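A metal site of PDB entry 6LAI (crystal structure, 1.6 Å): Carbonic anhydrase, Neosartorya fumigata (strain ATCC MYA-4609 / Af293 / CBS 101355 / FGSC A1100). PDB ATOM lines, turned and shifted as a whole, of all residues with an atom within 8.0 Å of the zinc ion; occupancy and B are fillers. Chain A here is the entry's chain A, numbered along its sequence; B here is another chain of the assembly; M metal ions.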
ATOM      1  N   GLY A  33      12.282   4.050 -20.985  1.00  0.00           N
ATOM      2  CA  GLY A  33      10.956   3.668 -20.514  1.00  0.00           C
ATOM      3  C   GLY A  33      11.064   2.438 -19.661  1.00  0.00           C
ATOM      4  O   GLY A  33      12.145   1.865 -19.490  1.00  0.00           O
ATOM      5  N   CYS A  34       9.944   2.024 -19.104  1.00  0.00           N
ATOM      6  CA  CYS A  34       9.869   0.859 -18.193  1.00  0.00           C
ATOM      7  C   CYS A  34       9.412  -0.427 -18.887  1.00  0.00           C
ATOM      8  O   CYS A  34       8.463  -0.419 -19.675  1.00  0.00           O
ATOM      9  CB  CYS A  34       8.978   1.187 -17.017  1.00  0.00           C
ATOM     10  SG  CYS A  34       8.878  -0.100 -15.737  1.00  0.00           S
ATOM     11  N   SER A  35      10.060  -1.508 -18.482  1.00  0.00           N
ATOM     12  CA  SER A  35       9.750  -2.874 -18.923  1.00  0.00           C
ATOM     13  C   SER A  35       8.318  -3.308 -18.641  1.00  0.00           C
ATOM     14  O   SER A  35       7.808  -4.059 -19.492  1.00  0.00           O
ATOM     15  CB  SER A  35      10.713  -3.866 -18.292  1.00  0.00           C
ATOM     16  OG  SER A  35      12.030  -3.528 -18.658  1.00  0.00           O
ATOM     17  N   ASP A  36       7.616  -2.769 -17.635  1.00  0.00           N
ATOM     18  CA  ASP A  36       6.186  -3.154 -17.442  1.00  0.00           C
ATOM     19  C   ASP A  36       5.237  -2.073 -17.974  1.00  0.00           C
ATOM     20  O   ASP A  36       4.018  -2.159 -17.743  1.00  0.00           O
ATOM     21  CB  ASP A  36       5.880  -3.564 -16.005  1.00  0.00           C
ATOM     22  CG  ASP A  36       5.916  -2.493 -14.944  1.00  0.00           C
ATOM     23  OD1 ASP A  36       5.865  -1.338 -15.314  1.00  0.00           O
ATOM     24  OD2 ASP A  36       6.074  -2.855 -13.776  1.00  0.00           O
ATOM     25  N   SER A  37       5.762  -1.082 -18.696  1.00  0.00           N
ATOM     26  CA  SER A  37       4.947  -0.230 -19.570  1.00  0.00           C
ATOM     27  C   SER A  37       4.861  -0.913 -20.918  1.00  0.00           C
ATOM     28  O   SER A  37       4.816  -2.180 -20.964  1.00  0.00           O
ATOM     29  CB  SER A  37       5.518   1.177 -19.645  1.00  0.00           C
ATOM     30  OG  SER A  37       4.603   2.015 -20.327  1.00  0.00           O
ATOM     31  N   GLY A  38       4.703  -0.175 -21.980  1.00  0.00           N
ATOM     32  CA  GLY A  38       4.644  -0.785 -23.303  1.00  0.00           C
ATOM     33  C   GLY A  38       4.567   0.232 -24.406  1.00  0.00           C
ATOM     34  O   GLY A  38       4.765   1.452 -24.158  1.00  0.00           O
ATOM     35  N   GLU A  41       2.785   3.957 -24.631  1.00  0.00           N
ATOM     36  CA  GLU A  41       3.344   5.214 -24.137  1.00  0.00           C
ATOM     37  C   GLU A  41       3.936   5.993 -25.307  1.00  0.00           C
ATOM     38  O   GLU A  41       3.907   7.229 -25.241  1.00  0.00           O
ATOM     39  CB  GLU A  41       4.340   5.046 -23.011  1.00  0.00           C
ATOM     40  CG  GLU A  41       5.680   4.464 -23.429  1.00  0.00           C
ATOM     41  CD  GLU A  41       6.607   4.198 -22.257  1.00  0.00           C
ATOM     42  OE1 GLU A  41       6.124   4.039 -21.110  1.00  0.00           O
ATOM     43  OE2 GLU A  41       7.841   4.161 -22.515  1.00  0.00           O
ATOM     44  N   ARG A  56      14.619   0.189 -22.635  1.00  0.00           N
ATOM     45  CA  ARG A  56      13.450  -0.152 -21.802  1.00  0.00           C
ATOM     46  C   ARG A  56      13.925  -1.075 -20.697  1.00  0.00           C
ATOM     47  O   ARG A  56      14.437  -2.180 -20.998  1.00  0.00           O
ATOM     48  CB  ARG A  56      12.305  -0.726 -22.620  1.00  0.00           C
ATOM     49  CG  ARG A  56      11.014  -0.801 -21.849  1.00  0.00           C
ATOM     50  CD  ARG A  56       9.805  -1.147 -22.661  1.00  0.00           C
ATOM     51  NE  ARG A  56       9.474  -0.108 -23.597  1.00  0.00           N
ATOM     52  CZ  ARG A  56       8.948   1.075 -23.276  1.00  0.00           C
ATOM     53  NH1 ARG A  56       8.547   1.301 -22.034  1.00  0.00           N
ATOM     54  NH2 ARG A  56       8.722   1.987 -24.198  1.00  0.00           N
ATOM     55  N   SER A  57      13.799  -0.586 -19.484  1.00  0.00           N
ATOM     56  CA  SER A  57      14.537  -1.124 -18.308  1.00  0.00           C
ATOM     57  C   SER A  57      13.648  -1.201 -17.087  1.00  0.00           C
ATOM     58  O   SER A  57      12.518  -0.643 -17.069  1.00  0.00           O
ATOM     59  CB  SER A  57      15.688  -0.190 -17.997  1.00  0.00           C
ATOM     60  OG  SER A  57      15.183   1.093 -17.595  1.00  0.00           O
ATOM     61  N   LEU A  58      14.113  -1.861 -16.052  1.00  0.00           N
ATOM     62  CA  LEU A  58      13.359  -1.891 -14.759  1.00  0.00           C
ATOM     63  C   LEU A  58      13.113  -0.469 -14.252  1.00  0.00           C
ATOM     64  O   LEU A  58      14.080   0.245 -13.961  1.00  0.00           O
ATOM     65  CB  LEU A  58      14.172  -2.671 -13.735  1.00  0.00           C
ATOM     66  CG  LEU A  58      14.434  -4.128 -14.071  1.00  0.00           C
ATOM     67  CD1 LEU A  58      15.374  -4.718 -13.032  1.00  0.00           C
ATOM     68  CD2 LEU A  58      13.179  -4.918 -14.127  1.00  0.00           C
ATOM     69  N   GLY A  59      11.853  -0.112 -14.085  1.00  0.00           N
ATOM     70  CA  GLY A  59      11.448   1.181 -13.487  1.00  0.00           C
ATOM     71  C   GLY A  59      11.936   2.389 -14.273  1.00  0.00           C
ATOM     72  O   GLY A  59      12.026   3.470 -13.650  1.00  0.00           O
ATOM     73  N   ASN A  60      12.207   2.255 -15.576  1.00  0.00           N
ATOM     74  CA  ASN A  60      12.686   3.392 -16.400  1.00  0.00           C
ATOM     75  C   ASN A  60      13.834   4.061 -15.650  1.00  0.00           C
ATOM     76  O   ASN A  60      13.946   5.310 -15.608  1.00  0.00           O
ATOM     77  CB  ASN A  60      11.546   4.336 -16.832  1.00  0.00           C
ATOM     78  CG  ASN A  60      10.654   4.867 -15.733  1.00  0.00           C
ATOM     79  OD1 ASN A  60       9.645   4.214 -15.475  1.00  0.00           O
ATOM     80  ND2 ASN A  60      10.991   5.991 -15.096  1.00  0.00           N
ATOM     81  N   CYS A  87      10.665   8.426 -19.302  1.00  0.00           N
ATOM     82  CA  CYS A  87       9.199   8.303 -19.313  1.00  0.00           C
ATOM     83  C   CYS A  87       8.814   7.273 -18.248  1.00  0.00           C
ATOM     84  O   CYS A  87       9.106   6.078 -18.377  1.00  0.00           O
ATOM     85  CB  CYS A  87       8.726   7.855 -20.676  1.00  0.00           C
ATOM     86  SG  CYS A  87       6.910   7.815 -20.764  1.00  0.00           S
ATOM     87  N   GLY A  88       8.207   7.743 -17.163  1.00  0.00           N
ATOM     88  CA  GLY A  88       7.552   6.869 -16.191  1.00  0.00           C
ATOM     89  C   GLY A  88       6.109   6.626 -16.582  1.00  0.00           C
ATOM     90  O   GLY A  88       5.631   7.210 -17.572  1.00  0.00           O
ATOM     91  N   HIS A  89       5.390   5.792 -15.822  1.00  0.00           N
ATOM     92  CA  HIS A  89       3.994   5.528 -16.220  1.00  0.00           C
ATOM     93  C   HIS A  89       3.180   5.185 -14.972  1.00  0.00           C
ATOM     94  O   HIS A  89       3.616   4.367 -14.169  1.00  0.00           O
ATOM     95  CB  HIS A  89       3.891   4.429 -17.284  1.00  0.00           C
ATOM     96  CG  HIS A  89       4.421   3.100 -16.849  1.00  0.00           C
ATOM     97  ND1 HIS A  89       3.601   1.988 -16.769  1.00  0.00           N
ATOM     98  CD2 HIS A  89       5.623   2.738 -16.329  1.00  0.00           C
ATOM     99  CE1 HIS A  89       4.347   0.981 -16.294  1.00  0.00           C
ATOM    100  NE2 HIS A  89       5.548   1.416 -15.934  1.00  0.00           N
ATOM    101  N   TYR A  90       2.026   5.788 -14.847  1.00  0.00           N
ATOM    102  CA  TYR A  90       1.142   5.474 -13.720  1.00  0.00           C
ATOM    103  C   TYR A  90       0.706   4.029 -13.828  1.00  0.00           C
ATOM    104  O   TYR A  90       0.447   3.536 -14.944  1.00  0.00           O
ATOM    105  CB  TYR A  90      -0.039   6.446 -13.737  1.00  0.00           C
ATOM    106  CG  TYR A  90       0.350   7.884 -13.545  1.00  0.00           C
ATOM    107  CD1 TYR A  90       1.012   8.287 -12.397  1.00  0.00           C
ATOM    108  CD2 TYR A  90      -0.029   8.855 -14.451  1.00  0.00           C
ATOM    109  CE1 TYR A  90       1.366   9.599 -12.169  1.00  0.00           C
ATOM    110  CE2 TYR A  90       0.279  10.189 -14.216  1.00  0.00           C
ATOM    111  CZ  TYR A  90       0.938  10.558 -13.056  1.00  0.00           C
ATOM    112  OH  TYR A  90       1.244  11.898 -12.939  1.00  0.00           O
ATOM    113  N   GLY A  91       0.642   3.404 -12.672  1.00  0.00           N
ATOM    114  CA  GLY A  91       0.316   1.973 -12.593  1.00  0.00           C
ATOM    115  C   GLY A  91       1.524   1.082 -12.668  1.00  0.00           C
ATOM    116  O   GLY A  91       1.359  -0.159 -12.553  1.00  0.00           O
ATOM    117  N   CYS A  92       2.714   1.668 -12.777  1.00  0.00           N
ATOM    118  CA  CYS A  92       3.989   0.903 -12.719  1.00  0.00           C
ATOM    119  C   CYS A  92       4.007  -0.063 -11.538  1.00  0.00           C
ATOM    120  O   CYS A  92       3.653   0.336 -10.422  1.00  0.00           O
ATOM    121  CB  CYS A  92       5.143   1.884 -12.607  1.00  0.00           C
ATOM    122  SG  CYS A  92       6.796   1.152 -12.759  1.00  0.00           S
ATOM    123  N   HIS A  93       4.401  -1.320 -11.730  1.00  0.00           N
ATOM    124  CA  HIS A  93       4.501  -2.280 -10.612  1.00  0.00           C
ATOM    125  C   HIS A  93       5.852  -2.231  -9.935  1.00  0.00           C
ATOM    126  O   HIS A  93       6.005  -2.708  -8.798  1.00  0.00           O
ATOM    127  CB  HIS A  93       4.178  -3.700 -11.079  1.00  0.00           C
ATOM    128  CG  HIS A  93       2.804  -3.806 -11.661  1.00  0.00           C
ATOM    129  ND1 HIS A  93       1.668  -3.685 -10.896  1.00  0.00           N
ATOM    130  CD2 HIS A  93       2.405  -4.042 -12.929  1.00  0.00           C
ATOM    131  CE1 HIS A  93       0.612  -3.841 -11.670  1.00  0.00           C
ATOM    132  NE2 HIS A  93       1.032  -4.071 -12.916  1.00  0.00           N
ATOM    133  N   ILE A  94       6.860  -1.685 -10.599  1.00  0.00           N
ATOM    134  CA  ILE A  94       8.228  -1.589 -10.036  1.00  0.00           C
ATOM    135  C   ILE A  94       8.310  -0.373  -9.133  1.00  0.00           C
ATOM    136  O   ILE A  94       8.757  -0.519  -7.930  1.00  0.00           O
ATOM    137  CB  ILE A  94       9.239  -1.588 -11.196  1.00  0.00           C
ATOM    138  CG1 ILE A  94       9.189  -2.940 -11.915  1.00  0.00           C
ATOM    139  CG2 ILE A  94      10.637  -1.258 -10.678  1.00  0.00           C
ATOM    140  CD1 ILE A  94       9.902  -3.049 -13.244  1.00  0.00           C
ATOM    141  N   ALA A  95       7.988   0.817  -9.656  1.00  0.00           N
ATOM    142  CA  ALA A  95       8.005   2.053  -8.845  1.00  0.00           C
ATOM    143  C   ALA A  95       6.646   2.116  -8.118  1.00  0.00           C
ATOM    144  O   ALA A  95       5.815   2.930  -8.492  1.00  0.00           O
ATOM    145  CB  ALA A  95       8.257   3.267  -9.684  1.00  0.00           C
ATOM    146  N   SER A  96       6.436   1.244  -7.138  1.00  0.00           N
ATOM    147  CA  SER A  96       5.156   1.153  -6.403  1.00  0.00           C
ATOM    148  C   SER A  96       5.398   0.607  -5.003  1.00  0.00           C
ATOM    149  O   SER A  96       6.449  -0.023  -4.772  1.00  0.00           O
ATOM    150  CB  SER A  96       4.068   0.392  -7.137  1.00  0.00           C
ATOM    151  OG  SER A  96       4.157  -1.002  -6.963  1.00  0.00           O
ATOM    152  N   VAL A 135       5.979   7.249  -8.762  1.00  0.00           N
ATOM    153  CA  VAL A 135       6.313   7.218 -10.205  1.00  0.00           C
ATOM    154  C   VAL A 135       6.879   8.590 -10.610  1.00  0.00           C
ATOM    155  O   VAL A 135       7.858   8.601 -11.283  1.00  0.00           O
ATOM    156  CB  VAL A 135       5.071   6.885 -11.042  1.00  0.00           C
ATOM    157  CG1 VAL A 135       5.230   7.243 -12.504  1.00  0.00           C
ATOM    158  CG2 VAL A 135       4.663   5.436 -10.885  1.00  0.00           C
ATOM    159  N   ASN A 138      10.347   9.238  -9.004  1.00  0.00           N
ATOM    160  CA  ASN A 138      11.391   8.419  -9.642  1.00  0.00           C
ATOM    161  C   ASN A 138      11.798   9.109 -10.948  1.00  0.00           C
ATOM    162  O   ASN A 138      12.994   9.200 -11.248  1.00  0.00           O
ATOM    163  CB  ASN A 138      10.861   6.988  -9.820  1.00  0.00           C
ATOM    164  CG  ASN A 138      11.881   6.092 -10.462  1.00  0.00           C
ATOM    165  OD1 ASN A 138      13.009   5.988 -10.012  1.00  0.00           O
ATOM    166  ND2 ASN A 138      11.484   5.425 -11.556  1.00  0.00           N
ATOM    167  N   PHE B  53       6.534  -8.130 -21.142  1.00  0.00           N
ATOM    168  CA  PHE B  53       7.476  -7.472 -20.214  1.00  0.00           C
ATOM    169  C   PHE B  53       8.760  -7.326 -21.033  1.00  0.00           C
ATOM    170  O   PHE B  53       9.427  -8.322 -21.267  1.00  0.00           O
ATOM    171  CB  PHE B  53       7.684  -8.310 -18.956  1.00  0.00           C
ATOM    172  CG  PHE B  53       8.557  -7.694 -17.919  1.00  0.00           C
ATOM    173  CD1 PHE B  53       8.110  -6.645 -17.110  1.00  0.00           C
ATOM    174  CD2 PHE B  53       9.882  -8.105 -17.797  1.00  0.00           C
ATOM    175  CE1 PHE B  53       8.935  -6.128 -16.126  1.00  0.00           C
ATOM    176  CE2 PHE B  53      10.699  -7.592 -16.804  1.00  0.00           C
ATOM    177  CZ  PHE B  53      10.227  -6.581 -15.983  1.00  0.00           C
ATOM    178  N   TYR B  74      14.199 -10.538 -11.815  1.00  0.00           N
ATOM    179  CA  TYR B  74      12.876  -9.975 -11.560  1.00  0.00           C
ATOM    180  C   TYR B  74      11.834 -10.774 -12.348  1.00  0.00           C
ATOM    181  O   TYR B  74      10.789 -11.173 -11.847  1.00  0.00           O
ATOM    182  CB  TYR B  74      12.836  -8.489 -11.942  1.00  0.00           C
ATOM    183  CG  TYR B  74      11.511  -7.836 -11.671  1.00  0.00           C
ATOM    184  CD1 TYR B  74      11.157  -7.440 -10.386  1.00  0.00           C
ATOM    185  CD2 TYR B  74      10.561  -7.657 -12.670  1.00  0.00           C
ATOM    186  CE1 TYR B  74       9.934  -6.860 -10.162  1.00  0.00           C
ATOM    187  CE2 TYR B  74       9.341  -7.063 -12.448  1.00  0.00           C
ATOM    188  CZ  TYR B  74       9.017  -6.653 -11.180  1.00  0.00           C
ATOM    189  OH  TYR B  74       7.755  -6.119 -10.961  1.00  0.00           O
HETATM  190 ZN    ZN M   1       6.861   0.310 -14.868  1.00  0.00          ZN
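The side-chain sulfur (SG) of Cys 34 lies close to the backbone NH (N) of Gly 59, at 3.4 Å.
The side-chain sulfur (SG) of Cys 92 sits close to the backbone NH (N) of Ile 94 (3.6 Å).
The backbone NH (N) of His 93 sits at hydrogen-bond distance from the side-chain carboxylate (OD2) of Asp 36 (3.1 Å).
N of Ile 94 sits at hydrogen-bond distance from OD2 of Asp 36.
The side-chain sulfur (SG) of Cys 92 sits close to the backbone NH (N) of Ala 95 (3.3 Å).
The backbone carbonyl oxygen (O) of Cys 34 sits at hydrogen-bond distance from the guanidinium group (NH1) of Arg 56.
Four residues have an atom within 4 Å of the zinc ion: Cys 34, Asp 36, His 89 and Cys 92.
OD1 of Asp 36 binds the zinc ion, at 2.0 Å.
The zinc ion is bound by NE2 of His 89.
The zinc ion is bound by SG of Cys 34.
The zinc ion is bound by the side-chain sulfur (SG) of Cys 92.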
